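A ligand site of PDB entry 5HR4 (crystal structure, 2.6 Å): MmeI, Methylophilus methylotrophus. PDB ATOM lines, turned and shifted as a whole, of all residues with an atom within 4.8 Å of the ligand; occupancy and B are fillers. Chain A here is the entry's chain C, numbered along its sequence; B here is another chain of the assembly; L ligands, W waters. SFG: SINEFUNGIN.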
ATOM      1  N   PHE A 299      31.533  11.305  -3.906  1.00  0.00           N
ATOM      2  CA  PHE A 299      30.301  12.079  -4.000  1.00  0.00           C
ATOM      3  C   PHE A 299      29.825  12.188  -5.442  1.00  0.00           C
ATOM      4  O   PHE A 299      28.649  11.961  -5.742  1.00  0.00           O
ATOM      5  CB  PHE A 299      30.582  13.447  -3.363  1.00  0.00           C
ATOM      6  CG  PHE A 299      29.604  14.530  -3.714  1.00  0.00           C
ATOM      7  CD1 PHE A 299      28.247  14.285  -3.819  1.00  0.00           C
ATOM      8  CD2 PHE A 299      30.065  15.830  -3.897  1.00  0.00           C
ATOM      9  CE1 PHE A 299      27.356  15.296  -4.145  1.00  0.00           C
ATOM     10  CE2 PHE A 299      29.178  16.858  -4.220  1.00  0.00           C
ATOM     11  CZ  PHE A 299      27.822  16.589  -4.333  1.00  0.00           C
ATOM     12  N   LEU A 311      21.807  19.627  -9.619  1.00  0.00           N
ATOM     13  CA  LEU A 311      22.091  20.008  -8.245  1.00  0.00           C
ATOM     14  C   LEU A 311      23.383  20.798  -8.128  1.00  0.00           C
ATOM     15  O   LEU A 311      23.751  21.198  -7.010  1.00  0.00           O
ATOM     16  CB  LEU A 311      22.151  18.775  -7.344  1.00  0.00           C
ATOM     17  CG  LEU A 311      20.778  18.101  -7.266  1.00  0.00           C
ATOM     18  CD1 LEU A 311      20.766  17.015  -6.235  1.00  0.00           C
ATOM     19  CD2 LEU A 311      19.671  19.137  -6.988  1.00  0.00           C
ATOM     20  N   GLY A 312      24.058  21.064  -9.232  1.00  0.00           N
ATOM     21  CA  GLY A 312      25.396  21.623  -9.162  1.00  0.00           C
ATOM     22  C   GLY A 312      26.360  20.793  -8.347  1.00  0.00           C
ATOM     23  O   GLY A 312      27.140  21.364  -7.563  1.00  0.00           O
ATOM     24  N   ALA A 313      26.342  19.468  -8.506  1.00  0.00           N
ATOM     25  CA  ALA A 313      27.111  18.581  -7.620  1.00  0.00           C
ATOM     26  C   ALA A 313      28.575  18.462  -8.068  1.00  0.00           C
ATOM     27  O   ALA A 313      29.056  17.413  -8.505  1.00  0.00           O
ATOM     28  CB  ALA A 313      26.456  17.224  -7.531  1.00  0.00           C
ATOM     29  N   HIS A 314      29.315  19.550  -7.893  1.00  0.00           N
ATOM     30  CA  HIS A 314      30.690  19.627  -8.341  1.00  0.00           C
ATOM     31  C   HIS A 314      31.568  19.971  -7.154  1.00  0.00           C
ATOM     32  O   HIS A 314      31.399  21.025  -6.543  1.00  0.00           O
ATOM     33  CB  HIS A 314      30.837  20.642  -9.453  1.00  0.00           C
ATOM     34  CG  HIS A 314      30.257  20.171 -10.738  1.00  0.00           C
ATOM     35  ND1 HIS A 314      29.147  20.748 -11.317  1.00  0.00           N
ATOM     36  CD2 HIS A 314      30.585  19.119 -11.522  1.00  0.00           C
ATOM     37  CE1 HIS A 314      28.859  20.100 -12.429  1.00  0.00           C
ATOM     38  NE2 HIS A 314      29.715  19.112 -12.578  1.00  0.00           N
ATOM     39  N   TYR A 315      32.469  19.050  -6.800  1.00  0.00           N
ATOM     40  CA  TYR A 315      33.255  19.243  -5.600  1.00  0.00           C
ATOM     41  C   TYR A 315      34.315  20.322  -5.839  1.00  0.00           C
ATOM     42  O   TYR A 315      34.786  20.522  -6.964  1.00  0.00           O
ATOM     43  CB  TYR A 315      33.893  17.925  -5.166  1.00  0.00           C
ATOM     44  CG  TYR A 315      35.322  17.718  -5.607  1.00  0.00           C
ATOM     45  CD1 TYR A 315      36.374  18.300  -4.906  1.00  0.00           C
ATOM     46  CD2 TYR A 315      35.614  16.908  -6.689  1.00  0.00           C
ATOM     47  CE1 TYR A 315      37.678  18.114  -5.291  1.00  0.00           C
ATOM     48  CE2 TYR A 315      36.915  16.713  -7.084  1.00  0.00           C
ATOM     49  CZ  TYR A 315      37.953  17.322  -6.378  1.00  0.00           C
ATOM     50  OH  TYR A 315      39.283  17.149  -6.771  1.00  0.00           O
ATOM     51  N   THR A 316      34.678  21.008  -4.762  1.00  0.00           N
ATOM     52  CA  THR A 316      35.584  22.154  -4.819  1.00  0.00           C
ATOM     53  C   THR A 316      37.003  21.733  -4.473  1.00  0.00           C
ATOM     54  O   THR A 316      37.238  21.124  -3.418  1.00  0.00           O
ATOM     55  CB  THR A 316      35.114  23.275  -3.890  1.00  0.00           C
ATOM     56  OG1 THR A 316      33.716  23.514  -4.112  1.00  0.00           O
ATOM     57  CG2 THR A 316      35.872  24.541  -4.186  1.00  0.00           C
ATOM     58  N   ILE A 321      39.211  26.241  -2.427  1.00  0.00           N
ATOM     59  CA  ILE A 321      38.874  26.520  -1.026  1.00  0.00           C
ATOM     60  C   ILE A 321      39.969  27.359  -0.346  1.00  0.00           C
ATOM     61  O   ILE A 321      39.679  28.271   0.440  1.00  0.00           O
ATOM     62  CB  ILE A 321      38.611  25.201  -0.277  1.00  0.00           C
ATOM     63  CG1 ILE A 321      37.465  24.442  -0.947  1.00  0.00           C
ATOM     64  CG2 ILE A 321      38.301  25.440   1.181  1.00  0.00           C
ATOM     65  CD1 ILE A 321      37.191  23.064  -0.350  1.00  0.00           C
ATOM     66  N   ASP A 361      28.731  26.006   6.274  1.00  0.00           N
ATOM     67  CA  ASP A 361      28.642  25.871   4.815  1.00  0.00           C
ATOM     68  C   ASP A 361      27.217  25.492   4.388  1.00  0.00           C
ATOM     69  O   ASP A 361      26.853  24.309   4.406  1.00  0.00           O
ATOM     70  CB  ASP A 361      29.651  24.829   4.317  1.00  0.00           C
ATOM     71  CG  ASP A 361      29.734  24.746   2.787  1.00  0.00           C
ATOM     72  OD1 ASP A 361      28.881  25.337   2.054  1.00  0.00           O
ATOM     73  OD2 ASP A 361      30.660  24.039   2.276  1.00  0.00           O
ATOM     74  N   PRO A 362      26.405  26.475   3.929  1.00  0.00           N
ATOM     75  CA  PRO A 362      24.971  26.229   3.697  1.00  0.00           C
ATOM     76  C   PRO A 362      24.654  25.560   2.363  1.00  0.00           C
ATOM     77  O   PRO A 362      23.579  25.771   1.809  1.00  0.00           O
ATOM     78  CB  PRO A 362      24.366  27.643   3.745  1.00  0.00           C
ATOM     79  CG  PRO A 362      25.556  28.621   3.687  1.00  0.00           C
ATOM     80  CD  PRO A 362      26.801  27.823   3.502  1.00  0.00           C
ATOM     81  N   ALA A 363      25.589  24.759   1.856  1.00  0.00           N
ATOM     82  CA  ALA A 363      25.444  23.982   0.629  1.00  0.00           C
ATOM     83  C   ALA A 363      26.672  23.080   0.526  1.00  0.00           C
ATOM     84  O   ALA A 363      27.315  22.995  -0.524  1.00  0.00           O
ATOM     85  CB  ALA A 363      25.305  24.902  -0.589  1.00  0.00           C
ATOM     86  N   CYS A 364      26.981  22.384   1.616  1.00  0.00           N
ATOM     87  CA  CYS A 364      28.341  21.938   1.877  1.00  0.00           C
ATOM     88  C   CYS A 364      28.798  20.769   1.011  1.00  0.00           C
ATOM     89  O   CYS A 364      29.986  20.441   1.050  1.00  0.00           O
ATOM     90  CB  CYS A 364      28.482  21.568   3.355  1.00  0.00           C
ATOM     91  SG  CYS A 364      27.636  20.060   3.780  1.00  0.00           S
ATOM     92  N   GLY A 365      27.916  20.135   0.244  1.00  0.00           N
ATOM     93  CA  GLY A 365      28.373  19.008  -0.573  1.00  0.00           C
ATOM     94  C   GLY A 365      28.925  17.891   0.294  1.00  0.00           C
ATOM     95  O   GLY A 365      28.338  17.521   1.312  1.00  0.00           O
ATOM     96  N   CYS A 366      30.069  17.328  -0.095  1.00  0.00           N
ATOM     97  CA  CYS A 366      30.717  16.279   0.688  1.00  0.00           C
ATOM     98  C   CYS A 366      31.591  16.829   1.805  1.00  0.00           C
ATOM     99  O   CYS A 366      32.344  16.071   2.425  1.00  0.00           O
ATOM    100  CB  CYS A 366      31.555  15.371  -0.225  1.00  0.00           C
ATOM    101  SG  CYS A 366      33.160  16.112  -0.779  1.00  0.00           S
ATOM    102  N   GLY A 367      31.519  18.136   2.066  1.00  0.00           N
ATOM    103  CA  GLY A 367      32.142  18.712   3.252  1.00  0.00           C
ATOM    104  C   GLY A 367      33.542  19.251   3.080  1.00  0.00           C
ATOM    105  O   GLY A 367      34.213  19.513   4.078  1.00  0.00           O
ATOM    106  N   ASN A 368      34.007  19.470   1.844  1.00  0.00           N
ATOM    107  CA  ASN A 368      35.420  19.797   1.643  1.00  0.00           C
ATOM    108  C   ASN A 368      35.806  21.110   2.325  1.00  0.00           C
ATOM    109  O   ASN A 368      36.819  21.180   3.033  1.00  0.00           O
ATOM    110  CB  ASN A 368      35.732  19.818   0.150  1.00  0.00           C
ATOM    111  CG  ASN A 368      35.986  18.436  -0.384  1.00  0.00           C
ATOM    112  OD1 ASN A 368      36.563  17.614   0.322  1.00  0.00           O
ATOM    113  ND2 ASN A 368      35.546  18.152  -1.607  1.00  0.00           N
ATOM    114  N   PHE A 369      35.009  22.179   2.125  1.00  0.00           N
ATOM    115  CA  PHE A 369      35.251  23.425   2.847  1.00  0.00           C
ATOM    116  C   PHE A 369      35.406  23.182   4.345  1.00  0.00           C
ATOM    117  O   PHE A 369      36.290  23.779   4.985  1.00  0.00           O
ATOM    118  CB  PHE A 369      34.112  24.414   2.631  1.00  0.00           C
ATOM    119  CG  PHE A 369      34.184  25.125   1.337  1.00  0.00           C
ATOM    120  CD1 PHE A 369      34.984  26.236   1.195  1.00  0.00           C
ATOM    121  CD2 PHE A 369      33.432  24.696   0.273  1.00  0.00           C
ATOM    122  CE1 PHE A 369      35.051  26.903  -0.030  1.00  0.00           C
ATOM    123  CE2 PHE A 369      33.481  25.365  -0.929  1.00  0.00           C
ATOM    124  CZ  PHE A 369      34.301  26.461  -1.091  1.00  0.00           C
ATOM    125  N   ILE A 412      24.656  22.411   5.634  1.00  0.00           N
ATOM    126  CA  ILE A 412      23.372  22.007   5.057  1.00  0.00           C
ATOM    127  C   ILE A 412      23.619  21.393   3.675  1.00  0.00           C
ATOM    128  O   ILE A 412      24.347  21.973   2.851  1.00  0.00           O
ATOM    129  CB  ILE A 412      22.396  23.195   4.937  1.00  0.00           C
ATOM    130  CG1 ILE A 412      22.210  23.924   6.277  1.00  0.00           C
ATOM    131  CG2 ILE A 412      21.079  22.715   4.448  1.00  0.00           C
ATOM    132  CD1 ILE A 412      21.592  25.328   6.132  1.00  0.00           C
ATOM    133  N   GLU A 413      22.993  20.254   3.402  1.00  0.00           N
ATOM    134  CA  GLU A 413      23.217  19.512   2.161  1.00  0.00           C
ATOM    135  C   GLU A 413      21.960  18.710   1.799  1.00  0.00           C
ATOM    136  O   GLU A 413      21.413  17.996   2.641  1.00  0.00           O
ATOM    137  CB  GLU A 413      24.459  18.622   2.323  1.00  0.00           C
ATOM    138  CG  GLU A 413      24.643  17.507   1.306  1.00  0.00           C
ATOM    139  CD  GLU A 413      24.691  17.989  -0.156  1.00  0.00           C
ATOM    140  OE1 GLU A 413      25.289  19.055  -0.424  1.00  0.00           O
ATOM    141  OE2 GLU A 413      24.116  17.296  -1.055  1.00  0.00           O
ATOM    142  N   ILE A 414      21.500  18.841   0.559  1.00  0.00           N
ATOM    143  CA  ILE A 414      20.178  18.321   0.226  1.00  0.00           C
ATOM    144  C   ILE A 414      20.212  16.837  -0.120  1.00  0.00           C
ATOM    145  O   ILE A 414      19.204  16.147   0.051  1.00  0.00           O
ATOM    146  CB  ILE A 414      19.551  19.149  -0.920  1.00  0.00           C
ATOM    147  CG1 ILE A 414      18.039  18.907  -1.026  1.00  0.00           C
ATOM    148  CG2 ILE A 414      20.216  18.825  -2.254  1.00  0.00           C
ATOM    149  CD1 ILE A 414      17.336  19.929  -1.934  1.00  0.00           C
ATOM    150  N   GLU A 415      21.333  16.313  -0.607  1.00  0.00           N
ATOM    151  CA  GLU A 415      21.452  14.886  -0.886  1.00  0.00           C
ATOM    152  C   GLU A 415      22.042  14.175   0.322  1.00  0.00           C
ATOM    153  O   GLU A 415      23.005  14.657   0.930  1.00  0.00           O
ATOM    154  CB  GLU A 415      22.324  14.639  -2.118  1.00  0.00           C
ATOM    155  CG  GLU A 415      21.715  15.080  -3.444  1.00  0.00           C
ATOM    156  CD  GLU A 415      20.454  14.294  -3.863  1.00  0.00           C
ATOM    157  OE1 GLU A 415      20.522  13.049  -4.043  1.00  0.00           O
ATOM    158  OE2 GLU A 415      19.388  14.928  -4.045  1.00  0.00           O
ATOM    159  N   ALA A 459      18.959  18.733   4.394  1.00  0.00           N
ATOM    160  CA  ALA A 459      17.766  19.535   4.230  1.00  0.00           C
ATOM    161  C   ALA A 459      17.995  20.454   3.036  1.00  0.00           C
ATOM    162  O   ALA A 459      19.000  20.329   2.332  1.00  0.00           O
ATOM    163  CB  ALA A 459      17.455  20.318   5.501  1.00  0.00           C
ATOM    164  N   ASN A 460      17.082  21.382   2.823  1.00  0.00           N
ATOM    165  CA  ASN A 460      17.098  22.268   1.659  1.00  0.00           C
ATOM    166  C   ASN A 460      17.333  23.682   2.154  1.00  0.00           C
ATOM    167  O   ASN A 460      16.406  24.348   2.615  1.00  0.00           O
ATOM    168  CB  ASN A 460      15.783  22.157   0.874  1.00  0.00           C
ATOM    169  CG  ASN A 460      15.786  23.021  -0.368  1.00  0.00           C
ATOM    170  OD1 ASN A 460      16.102  24.216  -0.325  1.00  0.00           O
ATOM    171  ND2 ASN A 460      15.468  22.414  -1.497  1.00  0.00           N
ATOM    172  N   ALA A 461      18.580  24.145   2.024  1.00  0.00           N
ATOM    173  CA  ALA A 461      19.022  25.367   2.675  1.00  0.00           C
ATOM    174  C   ALA A 461      18.204  26.596   2.291  1.00  0.00           C
ATOM    175  O   ALA A 461      18.301  27.623   2.975  1.00  0.00           O
ATOM    176  CB  ALA A 461      20.483  25.634   2.329  1.00  0.00           C
ATOM    177  N   LEU A 462      17.428  26.522   1.211  1.00  0.00           N
ATOM    178  CA  LEU A 462      16.631  27.669   0.805  1.00  0.00           C
ATOM    179  C   LEU A 462      15.256  27.685   1.457  1.00  0.00           C
ATOM    180  O   LEU A 462      14.626  28.757   1.528  1.00  0.00           O
ATOM    181  CB  LEU A 462      16.488  27.700  -0.722  1.00  0.00           C
ATOM    182  CG  LEU A 462      17.800  27.787  -1.542  1.00  0.00           C
ATOM    183  CD1 LEU A 462      17.515  28.056  -2.996  1.00  0.00           C
ATOM    184  CD2 LEU A 462      18.743  28.832  -1.013  1.00  0.00           C
ATOM    185  N   ASN A 481      30.452  26.678  -1.680  1.00  0.00           N
ATOM    186  CA  ASN A 481      30.348  26.712  -3.135  1.00  0.00           C
ATOM    187  C   ASN A 481      28.954  26.248  -3.542  1.00  0.00           C
ATOM    188  O   ASN A 481      28.766  25.087  -3.950  1.00  0.00           O
ATOM    189  CB  ASN A 481      31.435  25.855  -3.773  1.00  0.00           C
ATOM    190  CG  ASN A 481      31.348  25.860  -5.275  1.00  0.00           C
ATOM    191  OD1 ASN A 481      30.783  26.774  -5.882  1.00  0.00           O
ATOM    192  ND2 ASN A 481      31.886  24.820  -5.889  1.00  0.00           N
ATOM    193  N   PRO A 482      27.967  27.137  -3.500  1.00  0.00           N
ATOM    194  CA  PRO A 482      26.570  26.754  -3.783  1.00  0.00           C
ATOM    195  C   PRO A 482      26.353  26.459  -5.263  1.00  0.00           C
ATOM    196  O   PRO A 482      27.106  26.940  -6.123  1.00  0.00           O
ATOM    197  CB  PRO A 482      25.771  27.999  -3.348  1.00  0.00           C
ATOM    198  CG  PRO A 482      26.714  28.821  -2.532  1.00  0.00           C
ATOM    199  CD  PRO A 482      28.083  28.538  -3.047  1.00  0.00           C
ATOM    200  N   PRO A 483      25.281  25.714  -5.591  1.00  0.00           N
ATOM    201  CA  PRO A 483      25.085  25.254  -6.974  1.00  0.00           C
ATOM    202  C   PRO A 483      24.752  26.376  -7.934  1.00  0.00           C
ATOM    203  O   PRO A 483      24.054  27.342  -7.581  1.00  0.00           O
ATOM    204  CB  PRO A 483      23.907  24.286  -6.846  1.00  0.00           C
ATOM    205  CG  PRO A 483      23.163  24.784  -5.679  1.00  0.00           C
ATOM    206  CD  PRO A 483      24.232  25.195  -4.708  1.00  0.00           C
ATOM    207  N   ASP A 497      11.849  27.928  -4.967  1.00  0.00           N
ATOM    208  CA  ASP A 497      12.854  28.286  -3.969  1.00  0.00           C
ATOM    209  C   ASP A 497      13.436  29.657  -4.253  1.00  0.00           C
ATOM    210  O   ASP A 497      13.509  30.503  -3.363  1.00  0.00           O
ATOM    211  CB  ASP A 497      13.981  27.243  -3.942  1.00  0.00           C
ATOM    212  CG  ASP A 497      13.548  25.925  -3.352  1.00  0.00           C
ATOM    213  OD1 ASP A 497      12.333  25.706  -3.163  1.00  0.00           O
ATOM    214  OD2 ASP A 497      14.443  25.083  -3.069  1.00  0.00           O
ATOM    215  N   TRP A 517      21.447  32.052  -2.374  1.00  0.00           N
ATOM    216  CA  TRP A 517      22.132  31.970  -1.079  1.00  0.00           C
ATOM    217  C   TRP A 517      22.579  33.336  -0.549  1.00  0.00           C
ATOM    218  O   TRP A 517      22.813  33.452   0.658  1.00  0.00           O
ATOM    219  CB  TRP A 517      23.356  31.046  -1.147  1.00  0.00           C
ATOM    220  CG  TRP A 517      23.010  29.601  -0.993  1.00  0.00           C
ATOM    221  CD1 TRP A 517      23.319  28.790   0.051  1.00  0.00           C
ATOM    222  CD2 TRP A 517      22.278  28.800  -1.920  1.00  0.00           C
ATOM    223  NE1 TRP A 517      22.827  27.521  -0.177  1.00  0.00           N
ATOM    224  CE2 TRP A 517      22.177  27.507  -1.378  1.00  0.00           C
ATOM    225  CE3 TRP A 517      21.694  29.058  -3.162  1.00  0.00           C
ATOM    226  CZ2 TRP A 517      21.523  26.468  -2.029  1.00  0.00           C
ATOM    227  CZ3 TRP A 517      21.040  28.019  -3.813  1.00  0.00           C
ATOM    228  CH2 TRP A 517      20.957  26.742  -3.251  1.00  0.00           C
ATOM    229  P    DA B   7      24.168  25.857 -16.769  1.00  0.00           P
ATOM    230  OP1  DA B   7      23.655  24.466 -16.864  1.00  0.00           O
ATOM    231  OP2  DA B   7      23.502  26.818 -15.858  1.00  0.00           O
ATOM    232  O5'  DA B   7      25.725  25.793 -16.488  1.00  0.00           O
ATOM    233  C5'  DA B   7      26.242  25.903 -15.223  1.00  0.00           C
ATOM    234  C4'  DA B   7      27.545  25.160 -15.229  1.00  0.00           C
ATOM    235  O4'  DA B   7      28.155  25.245 -13.939  1.00  0.00           O
ATOM    236  C3'  DA B   7      27.423  23.682 -15.558  1.00  0.00           C
ATOM    237  O3'  DA B   7      28.489  23.363 -16.424  1.00  0.00           O
ATOM    238  C2'  DA B   7      27.576  22.999 -14.198  1.00  0.00           C
ATOM    239  C1'  DA B   7      28.479  23.958 -13.456  1.00  0.00           C
ATOM    240  N9   DA B   7      28.280  24.046 -12.020  1.00  0.00           N
ATOM    241  C8   DA B   7      27.084  24.065 -11.368  1.00  0.00           C
ATOM    242  N7   DA B   7      27.198  24.223 -10.086  1.00  0.00           N
ATOM    243  C5   DA B   7      28.566  24.346  -9.876  1.00  0.00           C
ATOM    244  C6   DA B   7      29.345  24.552  -8.708  1.00  0.00           C
ATOM    245  N6   DA B   7      28.825  24.661  -7.482  1.00  0.00           N
ATOM    246  N1   DA B   7      30.675  24.629  -8.855  1.00  0.00           N
ATOM    247  C2   DA B   7      31.193  24.513 -10.074  1.00  0.00           C
ATOM    248  N3   DA B   7      30.569  24.328 -11.236  1.00  0.00           N
ATOM    249  C4   DA B   7      29.235  24.250 -11.065  1.00  0.00           C
HETATM  250  N   SFG L   1      31.521  22.421  -1.851  1.00  0.00           N
HETATM  251  CA  SFG L   1      31.146  21.027  -1.993  1.00  0.00           C
HETATM  252  C   SFG L   1      32.426  20.225  -2.099  1.00  0.00           C
HETATM  253  O   SFG L   1      33.523  20.831  -2.076  1.00  0.00           O
HETATM  254  OXT SFG L   1      32.412  18.977  -2.216  1.00  0.00           O
HETATM  255  CB  SFG L   1      30.291  20.837  -3.244  1.00  0.00           C
HETATM  256  CG  SFG L   1      29.111  21.789  -3.163  1.00  0.00           C
HETATM  257  CD  SFG L   1      28.450  21.758  -4.521  1.00  0.00           C
HETATM  258  NE  SFG L   1      29.212  22.659  -5.368  1.00  0.00           N
HETATM  259  C5' SFG L   1      26.981  22.176  -4.447  1.00  0.00           C
HETATM  260  C4' SFG L   1      26.112  21.338  -3.445  1.00  0.00           C
HETATM  261  O4' SFG L   1      25.014  21.982  -3.204  1.00  0.00           O
HETATM  262  C3' SFG L   1      25.641  19.983  -4.002  1.00  0.00           C
HETATM  263  O3' SFG L   1      26.254  19.015  -3.286  1.00  0.00           O
HETATM  264  C2' SFG L   1      24.089  19.968  -3.828  1.00  0.00           C
HETATM  265  O2' SFG L   1      23.607  18.657  -3.318  1.00  0.00           O
HETATM  266  C1' SFG L   1      23.869  20.875  -2.938  1.00  0.00           C
HETATM  267  N9  SFG L   1      22.638  21.576  -3.122  1.00  0.00           N
HETATM  268  C8  SFG L   1      22.064  21.950  -4.260  1.00  0.00           C
HETATM  269  N7  SFG L   1      20.951  22.633  -3.962  1.00  0.00           N
HETATM  270  C5  SFG L   1      20.845  22.672  -2.631  1.00  0.00           C
HETATM  271  C6  SFG L   1      19.886  23.225  -1.825  1.00  0.00           C
HETATM  272  N6  SFG L   1      18.670  23.966  -2.107  1.00  0.00           N
HETATM  273  N1  SFG L   1      19.984  23.152  -0.504  1.00  0.00           N
HETATM  274  C2  SFG L   1      21.041  22.510   0.041  1.00  0.00           C
HETATM  275  N3  SFG L   1      21.984  21.955  -0.759  1.00  0.00           N
HETATM  276  C4  SFG L   1      21.889  22.031  -2.105  1.00  0.00           C
HETATM  277  O   HOH W   1      30.085  24.423  -0.451  1.00  0.00           O
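Water W1 lies within hydrogen-bond range of N of Asn 481 (2.6 Å), OD2 of Asp 361 (2.8 Å), N of the ligand (2.8 Å) and O of Ala 363 (3.1 Å).
Residues that only touch the ligand: Phe 299, Leu 311, Tyr 315, Ala 363, Cys 364, Gly 365, Phe 369, Ala 459, Leu 462, Pro 483 and Trp 517.
Hydrophobic or aromatic side chains that line the ligand: Phe 299, Tyr 315, Ala 363, Phe 369, Ile 414, Ala 461, Leu 462, Pro 483 and Trp 517.
Within 4 Å of the ligand: Phe 299, Leu 311, Gly 312, His 314, Tyr 315, Thr 316, Ala 363, Cys 364, Gly 365, Cys 366, Asn 368, Phe 369, Glu 413, Ile 414, Ala 459, Asn 460, Ala 461, Leu 462, Asn 481, Pro 483, Trp 517 and DA 7 of chain B.
The nearest printed residue that does not touch the ligand is Glu 415 (4.05 Å).
The side-chain carboxylate (OE2) of Glu 413 is in hydrogen-bond range of an oxygen (O2') of the ligand.
The backbone carbonyl oxygen (O) of Asn 481 is in hydrogen-bond range of a nitrogen (NE) of the ligand, 2.8 Å away.
The side-chain amide nitrogen (ND2) of Asn 481 sits close to a nitrogen (NE) of the ligand (3.5 Å).
An oxygen (O) of the ligand sits at hydrogen-bond distance from the backbone NH of Thr 316.
N of the ligand sits at hydrogen-bond distance from OG1 of Thr 316, 3.3 Å away.
A nitrogen (NE) of the ligand is in hydrogen-bond range of N6 of DA 7 of chain B (2.9 Å).
The backbone carbonyl oxygen of His 314 is in hydrogen-bond range of a nitrogen (NE) of the ligand, 3.0 Å away.
N1 of the ligand lies within hydrogen-bond range of N of Ala 461, at 3.1 Å.
A nitrogen (N6) of the ligand sits at hydrogen-bond distance from the side-chain amide oxygen (OD1) of Asn 460 (3.1 Å).
NE of the ligand sits close to O of Gly 312, at 3.3 Å.
An oxygen (OXT) of the ligand is in hydrogen-bond range of the side-chain sulfur (SG) of Cys 366, at 3.3 Å.
An oxygen (OXT) of the ligand lies within hydrogen-bond range of the side-chain amide nitrogen (ND2) of Asn 368.
A nitrogen (N3) of the ligand sits at hydrogen-bond distance from the backbone NH of Ile 414, at 3.4 Å.
The backbone carbonyl oxygen of Glu 413 lies within hydrogen-bond range of the backbone NH of Ala 459.
The side-chain carboxylate (OE2) of Glu 413 sits at hydrogen-bond distance from the backbone NH (N) of Glu 415 (3.0 Å).
ND2 of Asn 481 sits at hydrogen-bond distance from N1 of DA 7 of chain B (3.2 Å).
N9 of DA 7 of chain B lies within hydrogen-bond range of a ring nitrogen (ND1) of His 314, at 3.5 Å.
The side-chain amide nitrogen (ND2) of Asn 460 lies within hydrogen-bond range of the side-chain carboxylate (OD2) of Asp 497 (3.3 Å).
The side-chain sulfur (SG) of Cys 366 lies within hydrogen-bond range of the side-chain amide nitrogen (ND2) of Asn 368, 3.2 Å away.
N of Cys 364 lies within hydrogen-bond range of O of Ile 412, at 2.9 Å.
O of Ala 459 sits close to N of Ile 414, at 3.4 Å.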
